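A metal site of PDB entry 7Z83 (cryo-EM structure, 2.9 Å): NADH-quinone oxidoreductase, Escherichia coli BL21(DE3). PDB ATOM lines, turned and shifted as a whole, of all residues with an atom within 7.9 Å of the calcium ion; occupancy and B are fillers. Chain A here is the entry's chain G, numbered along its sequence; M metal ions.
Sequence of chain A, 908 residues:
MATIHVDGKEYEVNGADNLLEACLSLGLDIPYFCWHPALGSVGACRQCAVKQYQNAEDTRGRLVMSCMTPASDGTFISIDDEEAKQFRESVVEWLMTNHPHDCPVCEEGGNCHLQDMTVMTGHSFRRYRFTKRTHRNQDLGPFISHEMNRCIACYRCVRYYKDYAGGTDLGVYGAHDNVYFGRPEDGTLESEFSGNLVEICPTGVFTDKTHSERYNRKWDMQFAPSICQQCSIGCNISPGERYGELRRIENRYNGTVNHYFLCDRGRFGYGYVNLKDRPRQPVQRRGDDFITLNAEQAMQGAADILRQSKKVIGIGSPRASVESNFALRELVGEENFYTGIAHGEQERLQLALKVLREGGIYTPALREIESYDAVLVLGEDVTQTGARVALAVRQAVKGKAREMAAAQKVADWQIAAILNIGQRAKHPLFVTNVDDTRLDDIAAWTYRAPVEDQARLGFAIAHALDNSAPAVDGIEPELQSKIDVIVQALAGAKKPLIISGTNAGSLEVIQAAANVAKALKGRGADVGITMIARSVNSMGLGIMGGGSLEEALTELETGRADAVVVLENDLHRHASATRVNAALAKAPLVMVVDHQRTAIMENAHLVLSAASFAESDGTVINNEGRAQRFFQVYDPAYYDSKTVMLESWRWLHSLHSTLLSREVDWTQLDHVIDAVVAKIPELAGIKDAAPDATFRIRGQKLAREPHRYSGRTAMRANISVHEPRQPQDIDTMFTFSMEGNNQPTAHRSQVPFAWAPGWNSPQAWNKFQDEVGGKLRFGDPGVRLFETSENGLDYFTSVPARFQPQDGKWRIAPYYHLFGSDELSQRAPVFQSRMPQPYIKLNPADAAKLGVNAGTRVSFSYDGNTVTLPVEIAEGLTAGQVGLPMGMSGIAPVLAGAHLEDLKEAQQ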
ATOM      1  N   GLU A 615     -23.777  19.939  18.211  1.00  0.00           N
ATOM      2  CA  GLU A 615     -23.327  18.703  18.823  1.00  0.00           C
ATOM      3  C   GLU A 615     -22.907  18.897  20.276  1.00  0.00           C
ATOM      4  O   GLU A 615     -22.247  18.035  20.847  1.00  0.00           O
ATOM      5  CB  GLU A 615     -22.168  18.116  18.019  1.00  0.00           C
ATOM      6  CG  GLU A 615     -22.453  18.023  16.534  1.00  0.00           C
ATOM      7  CD  GLU A 615     -21.424  18.733  15.686  1.00  0.00           C
ATOM      8  OE1 GLU A 615     -21.064  19.877  16.033  1.00  0.00           O
ATOM      9  OE2 GLU A 615     -21.001  18.157  14.672  1.00  0.00           O
ATOM     10  N   SER A 616     -23.320  20.006  20.892  1.00  0.00           N
ATOM     11  CA  SER A 616     -22.934  20.304  22.264  1.00  0.00           C
ATOM     12  C   SER A 616     -24.106  20.891  23.019  1.00  0.00           C
ATOM     13  O   SER A 616     -25.047  21.436  22.423  1.00  0.00           O
ATOM     14  CB  SER A 616     -21.744  21.269  22.327  1.00  0.00           C
ATOM     15  OG  SER A 616     -22.083  22.516  21.757  1.00  0.00           O
ATOM     16  N   ASP A 617     -24.052  20.754  24.331  1.00  0.00           N
ATOM     17  CA  ASP A 617     -24.960  21.408  25.253  1.00  0.00           C
ATOM     18  C   ASP A 617     -24.209  22.496  26.003  1.00  0.00           C
ATOM     19  O   ASP A 617     -23.006  22.374  26.246  1.00  0.00           O
ATOM     20  CB  ASP A 617     -25.565  20.407  26.245  1.00  0.00           C
ATOM     21  CG  ASP A 617     -25.888  19.079  25.614  1.00  0.00           C
ATOM     22  OD1 ASP A 617     -26.999  18.933  25.064  1.00  0.00           O
ATOM     23  OD2 ASP A 617     -25.024  18.176  25.653  1.00  0.00           O
ATOM     24  N   PHE A 631     -29.174  22.905  23.547  1.00  0.00           N
ATOM     25  CA  PHE A 631     -29.105  21.464  23.710  1.00  0.00           C
ATOM     26  C   PHE A 631     -28.499  20.825  22.468  1.00  0.00           C
ATOM     27  O   PHE A 631     -28.487  21.416  21.386  1.00  0.00           O
ATOM     28  CB  PHE A 631     -30.504  20.886  23.967  1.00  0.00           C
ATOM     29  CG  PHE A 631     -31.155  21.412  25.216  1.00  0.00           C
ATOM     30  CD1 PHE A 631     -31.904  22.578  25.199  1.00  0.00           C
ATOM     31  CD2 PHE A 631     -31.018  20.749  26.413  1.00  0.00           C
ATOM     32  CE1 PHE A 631     -32.497  23.064  26.336  1.00  0.00           C
ATOM     33  CE2 PHE A 631     -31.603  21.220  27.564  1.00  0.00           C
ATOM     34  CZ  PHE A 631     -32.348  22.381  27.526  1.00  0.00           C
ATOM     35  N   GLN A 632     -27.975  19.621  22.660  1.00  0.00           N
ATOM     36  CA  GLN A 632     -27.396  18.877  21.552  1.00  0.00           C
ATOM     37  C   GLN A 632     -28.477  18.436  20.577  1.00  0.00           C
ATOM     38  O   GLN A 632     -29.554  17.994  20.988  1.00  0.00           O
ATOM     39  CB  GLN A 632     -26.621  17.668  22.076  1.00  0.00           C
ATOM     40  CG  GLN A 632     -25.888  16.885  21.014  1.00  0.00           C
ATOM     41  CD  GLN A 632     -24.914  15.895  21.603  1.00  0.00           C
ATOM     42  OE1 GLN A 632     -24.544  15.994  22.770  1.00  0.00           O
ATOM     43  NE2 GLN A 632     -24.484  14.935  20.795  1.00  0.00           N
ATOM     44  N   VAL A 633     -28.207  18.569  19.286  1.00  0.00           N
ATOM     45  CA  VAL A 633     -29.161  18.149  18.264  1.00  0.00           C
ATOM     46  C   VAL A 633     -29.007  16.675  17.931  1.00  0.00           C
ATOM     47  O   VAL A 633     -29.999  15.940  17.846  1.00  0.00           O
ATOM     48  CB  VAL A 633     -29.011  19.030  17.005  1.00  0.00           C
ATOM     49  CG1 VAL A 633     -30.143  18.761  16.031  1.00  0.00           C
ATOM     50  CG2 VAL A 633     -28.959  20.482  17.384  1.00  0.00           C
ATOM     51  N   TYR A 634     -27.776  16.211  17.746  1.00  0.00           N
ATOM     52  CA  TYR A 634     -27.553  14.852  17.288  1.00  0.00           C
ATOM     53  C   TYR A 634     -26.226  14.349  17.829  1.00  0.00           C
ATOM     54  O   TYR A 634     -25.356  15.124  18.236  1.00  0.00           O
ATOM     55  CB  TYR A 634     -27.582  14.776  15.767  1.00  0.00           C
ATOM     56  CG  TYR A 634     -26.378  15.357  15.071  1.00  0.00           C
ATOM     57  CD1 TYR A 634     -26.229  16.728  14.920  1.00  0.00           C
ATOM     58  CD2 TYR A 634     -25.378  14.536  14.570  1.00  0.00           C
ATOM     59  CE1 TYR A 634     -25.131  17.263  14.284  1.00  0.00           C
ATOM     60  CE2 TYR A 634     -24.277  15.060  13.942  1.00  0.00           C
ATOM     61  CZ  TYR A 634     -24.156  16.425  13.803  1.00  0.00           C
ATOM     62  OH  TYR A 634     -23.051  16.945  13.167  1.00  0.00           O
ATOM     63  N   ASP A 635     -26.074  13.029  17.808  1.00  0.00           N
ATOM     64  CA  ASP A 635     -24.819  12.391  18.189  1.00  0.00           C
ATOM     65  C   ASP A 635     -23.936  12.282  16.958  1.00  0.00           C
ATOM     66  O   ASP A 635     -24.309  11.593  16.000  1.00  0.00           O
ATOM     67  CB  ASP A 635     -25.083  11.015  18.770  1.00  0.00           C
ATOM     68  CG  ASP A 635     -23.874  10.431  19.476  1.00  0.00           C
ATOM     69  OD1 ASP A 635     -22.924  11.189  19.773  1.00  0.00           O
ATOM     70  OD2 ASP A 635     -23.867   9.217  19.723  1.00  0.00           O
ATOM     71  N   PRO A 636     -22.766  12.928  16.933  1.00  0.00           N
ATOM     72  CA  PRO A 636     -21.887  12.817  15.752  1.00  0.00           C
ATOM     73  C   PRO A 636     -21.286  11.438  15.575  1.00  0.00           C
ATOM     74  O   PRO A 636     -20.862  11.106  14.464  1.00  0.00           O
ATOM     75  CB  PRO A 636     -20.803  13.865  16.017  1.00  0.00           C
ATOM     76  CG  PRO A 636     -21.244  14.632  17.205  1.00  0.00           C
ATOM     77  CD  PRO A 636     -22.202  13.807  17.966  1.00  0.00           C
ATOM     78  N   LEU A 646     -16.380  15.730  21.250  1.00  0.00           N
ATOM     79  CA  LEU A 646     -17.033  15.922  22.538  1.00  0.00           C
ATOM     80  C   LEU A 646     -17.246  17.407  22.784  1.00  0.00           C
ATOM     81  O   LEU A 646     -16.760  18.260  22.048  1.00  0.00           O
ATOM     82  CB  LEU A 646     -16.197  15.322  23.666  1.00  0.00           C
ATOM     83  CG  LEU A 646     -15.782  13.856  23.492  1.00  0.00           C
ATOM     84  CD1 LEU A 646     -14.824  13.447  24.583  1.00  0.00           C
ATOM     85  CD2 LEU A 646     -17.000  12.962  23.477  1.00  0.00           C
ATOM     86  N   GLU A 647     -18.003  17.694  23.829  1.00  0.00           N
ATOM     87  CA  GLU A 647     -18.187  19.064  24.280  1.00  0.00           C
ATOM     88  C   GLU A 647     -16.870  19.612  24.809  1.00  0.00           C
ATOM     89  O   GLU A 647     -16.015  18.878  25.294  1.00  0.00           O
ATOM     90  CB  GLU A 647     -19.251  19.130  25.361  1.00  0.00           C
ATOM     91  CG  GLU A 647     -20.666  18.891  24.858  1.00  0.00           C
ATOM     92  CD  GLU A 647     -21.092  17.442  24.944  1.00  0.00           C
ATOM     93  OE1 GLU A 647     -20.207  16.563  25.064  1.00  0.00           O
ATOM     94  OE2 GLU A 647     -22.310  17.176  24.882  1.00  0.00           O
ATOM     95  N   TRP A 649     -16.404  21.716  27.365  1.00  0.00           N
ATOM     96  CA  TRP A 649     -16.348  21.601  28.826  1.00  0.00           C
ATOM     97  C   TRP A 649     -16.057  20.173  29.251  1.00  0.00           C
ATOM     98  O   TRP A 649     -15.352  19.949  30.240  1.00  0.00           O
ATOM     99  CB  TRP A 649     -17.644  22.113  29.446  1.00  0.00           C
ATOM    100  CG  TRP A 649     -18.894  21.547  28.838  1.00  0.00           C
ATOM    101  CD1 TRP A 649     -19.627  22.093  27.836  1.00  0.00           C
ATOM    102  CD2 TRP A 649     -19.565  20.337  29.210  1.00  0.00           C
ATOM    103  NE1 TRP A 649     -20.714  21.301  27.545  1.00  0.00           N
ATOM    104  CE2 TRP A 649     -20.693  20.217  28.382  1.00  0.00           C
ATOM    105  CE3 TRP A 649     -19.324  19.350  30.167  1.00  0.00           C
ATOM    106  CZ2 TRP A 649     -21.570  19.145  28.470  1.00  0.00           C
ATOM    107  CZ3 TRP A 649     -20.195  18.287  30.255  1.00  0.00           C
ATOM    108  CH2 TRP A 649     -21.310  18.191  29.408  1.00  0.00           C
ATOM    109  N   ARG A 650     -16.570  19.189  28.499  1.00  0.00           N
ATOM    110  CA  ARG A 650     -16.256  17.794  28.775  1.00  0.00           C
ATOM    111  C   ARG A 650     -14.772  17.516  28.564  1.00  0.00           C
ATOM    112  O   ARG A 650     -14.131  16.870  29.400  1.00  0.00           O
ATOM    113  CB  ARG A 650     -17.113  16.890  27.891  1.00  0.00           C
ATOM    114  CG  ARG A 650     -16.941  15.415  28.157  1.00  0.00           C
ATOM    115  CD  ARG A 650     -18.143  14.626  27.667  1.00  0.00           C
ATOM    116  NE  ARG A 650     -19.094  14.364  28.742  1.00  0.00           N
ATOM    117  CZ  ARG A 650     -20.392  14.593  28.668  1.00  0.00           C
ATOM    118  NH1 ARG A 650     -20.942  15.122  27.586  1.00  0.00           N
ATOM    119  NH2 ARG A 650     -21.165  14.313  29.714  1.00  0.00           N
ATOM    120  N   LEU A 669     -23.341  17.313  32.575  1.00  0.00           N
ATOM    121  CA  LEU A 669     -23.491  18.742  32.324  1.00  0.00           C
ATOM    122  C   LEU A 669     -23.933  19.497  33.585  1.00  0.00           C
ATOM    123  O   LEU A 669     -23.445  20.601  33.867  1.00  0.00           O
ATOM    124  CB  LEU A 669     -24.475  18.994  31.184  1.00  0.00           C
ATOM    125  CG  LEU A 669     -24.944  20.429  30.953  1.00  0.00           C
ATOM    126  CD1 LEU A 669     -23.805  21.306  30.472  1.00  0.00           C
ATOM    127  CD2 LEU A 669     -26.103  20.470  29.973  1.00  0.00           C
ATOM    128  N   ARG A 704     -36.818  14.504  20.845  1.00  0.00           N
ATOM    129  CA  ARG A 704     -36.090  15.371  19.918  1.00  0.00           C
ATOM    130  C   ARG A 704     -36.675  15.307  18.520  1.00  0.00           C
ATOM    131  O   ARG A 704     -36.651  16.312  17.798  1.00  0.00           O
ATOM    132  CB  ARG A 704     -34.611  14.967  19.867  1.00  0.00           C
ATOM    133  CG  ARG A 704     -33.735  15.667  20.879  1.00  0.00           C
ATOM    134  CD  ARG A 704     -32.269  15.454  20.565  1.00  0.00           C
ATOM    135  NE  ARG A 704     -31.399  16.156  21.491  1.00  0.00           N
ATOM    136  CZ  ARG A 704     -30.981  15.671  22.645  1.00  0.00           C
ATOM    137  NH1 ARG A 704     -31.338  14.465  23.054  1.00  0.00           N
ATOM    138  NH2 ARG A 704     -30.198  16.414  23.423  1.00  0.00           N
ATOM    139  N   GLN A 728     -27.531   7.702  24.141  1.00  0.00           N
ATOM    140  CA  GLN A 728     -27.987   8.087  25.467  1.00  0.00           C
ATOM    141  C   GLN A 728     -27.562   9.522  25.747  1.00  0.00           C
ATOM    142  O   GLN A 728     -26.398   9.885  25.545  1.00  0.00           O
ATOM    143  CB  GLN A 728     -27.419   7.155  26.534  1.00  0.00           C
ATOM    144  CG  GLN A 728     -27.897   5.718  26.419  1.00  0.00           C
ATOM    145  CD  GLN A 728     -29.384   5.609  26.166  1.00  0.00           C
ATOM    146  OE1 GLN A 728     -29.824   5.136  25.122  1.00  0.00           O
ATOM    147  NE2 GLN A 728     -30.180   6.061  27.132  1.00  0.00           N
ATOM    148  N   ASP A 729     -28.511  10.339  26.191  1.00  0.00           N
ATOM    149  CA  ASP A 729     -28.265  11.730  26.549  1.00  0.00           C
ATOM    150  C   ASP A 729     -28.307  11.813  28.071  1.00  0.00           C
ATOM    151  O   ASP A 729     -29.368  12.048  28.659  1.00  0.00           O
ATOM    152  CB  ASP A 729     -29.277  12.652  25.906  1.00  0.00           C
ATOM    153  CG  ASP A 729     -28.898  14.115  26.033  1.00  0.00           C
ATOM    154  OD1 ASP A 729     -27.685  14.410  26.115  1.00  0.00           O
ATOM    155  OD2 ASP A 729     -29.814  14.964  26.055  1.00  0.00           O
ATOM    156  N   ILE A 730     -27.156  11.618  28.706  1.00  0.00           N
ATOM    157  CA  ILE A 730     -27.062  11.772  30.148  1.00  0.00           C
ATOM    158  C   ILE A 730     -26.940  13.236  30.566  1.00  0.00           C
ATOM    159  O   ILE A 730     -27.096  13.547  31.751  1.00  0.00           O
ATOM    160  CB  ILE A 730     -25.859  10.995  30.719  1.00  0.00           C
ATOM    161  CG1 ILE A 730     -24.546  11.588  30.222  1.00  0.00           C
ATOM    162  CG2 ILE A 730     -25.952   9.531  30.333  1.00  0.00           C
ATOM    163  CD1 ILE A 730     -23.370  11.314  31.131  1.00  0.00           C
ATOM    164  N   ASP A 731     -26.679  14.132  29.614  1.00  0.00           N
ATOM    165  CA  ASP A 731     -26.440  15.526  29.965  1.00  0.00           C
ATOM    166  C   ASP A 731     -27.741  16.287  30.202  1.00  0.00           C
ATOM    167  O   ASP A 731     -27.828  17.084  31.134  1.00  0.00           O
ATOM    168  CB  ASP A 731     -25.626  16.207  28.855  1.00  0.00           C
ATOM    169  CG  ASP A 731     -24.186  15.774  28.847  1.00  0.00           C
ATOM    170  OD1 ASP A 731     -23.577  15.692  29.931  1.00  0.00           O
ATOM    171  OD2 ASP A 731     -23.648  15.505  27.751  1.00  0.00           O
ATOM    172  N   THR A 732     -28.747  16.069  29.364  1.00  0.00           N
ATOM    173  CA  THR A 732     -29.975  16.858  29.382  1.00  0.00           C
ATOM    174  C   THR A 732     -31.193  15.942  29.526  1.00  0.00           C
ATOM    175  O   THR A 732     -31.083  14.726  29.631  1.00  0.00           O
ATOM    176  CB  THR A 732     -30.110  17.710  28.121  1.00  0.00           C
ATOM    177  OG1 THR A 732     -30.602  16.899  27.045  1.00  0.00           O
ATOM    178  CG2 THR A 732     -28.786  18.322  27.714  1.00  0.00           C
ATOM    179  N   PHE A 736     -32.520  11.171  22.348  1.00  0.00           N
ATOM    180  CA  PHE A 736     -32.222  11.112  20.918  1.00  0.00           C
ATOM    181  C   PHE A 736     -33.126  10.109  20.204  1.00  0.00           C
ATOM    182  O   PHE A 736     -32.642   9.237  19.490  1.00  0.00           O
ATOM    183  CB  PHE A 736     -30.764  10.727  20.682  1.00  0.00           C
ATOM    184  CG  PHE A 736     -29.788  11.800  21.059  1.00  0.00           C
ATOM    185  CD1 PHE A 736     -29.660  12.931  20.271  1.00  0.00           C
ATOM    186  CD2 PHE A 736     -28.995  11.672  22.186  1.00  0.00           C
ATOM    187  CE1 PHE A 736     -28.760  13.913  20.608  1.00  0.00           C
ATOM    188  CE2 PHE A 736     -28.095  12.654  22.523  1.00  0.00           C
ATOM    189  CZ  PHE A 736     -27.978  13.780  21.730  1.00  0.00           C
HETATM  190 CA    CA M   1     -24.304  15.719  25.283  1.00  0.00          CA
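The backbone NH of Gln 632 sits at hydrogen-bond distance from the backbone carbonyl oxygen of Ser 616 (3.5 Å). OD1 of Asp 731 lies within hydrogen-bond range of N of Leu 669 (3.1 Å). The side-chain amide nitrogen (NE2) of Gln 632 sits at hydrogen-bond distance from the backbone carbonyl oxygen (O) of Tyr 634, 2.7 Å away. The guanidinium group (NH2) of Arg 704 is in salt-bridge range of the side-chain carboxylate (OD2) of Asp 729 (3.0 Å). The guanidinium group of Arg 650 lies within salt-bridge range of the side-chain carboxylate of Asp 731 (2.8 Å). O of Gln 632 lies within hydrogen-bond range of NE of Arg 704, at 2.7 Å. The guanidinium group (NH1) of Arg 650 lies within salt-bridge range of the side-chain carboxylate (OE1) of Glu 647 (3.0 Å). NE1 of Trp 649 sits at hydrogen-bond distance from O of Asp 617, at 2.8 Å.
Asp 729 touches the calcium ion (OD1 to CA, 3.7 Å). Five residues have an atom within 4 Å of the calcium ion: Asp 617, Gln 632, Glu 647, Asp 729 and Asp 731. The nearest printed residue that does not touch the calcium ion is Arg 650 (4.1 Å).
OE2 of Glu 647 binds the calcium ion, 2.5 Å away. The side-chain amide oxygen (OE1) of Gln 632 is bound to the calcium ion (2.5 Å). The calcium ion is bound by OD2 of Asp 731 (2.6 Å). The calcium ion is bound by OD2 of Asp 617 (2.6 Å). The calcium ion has four donor atoms within binding distance.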
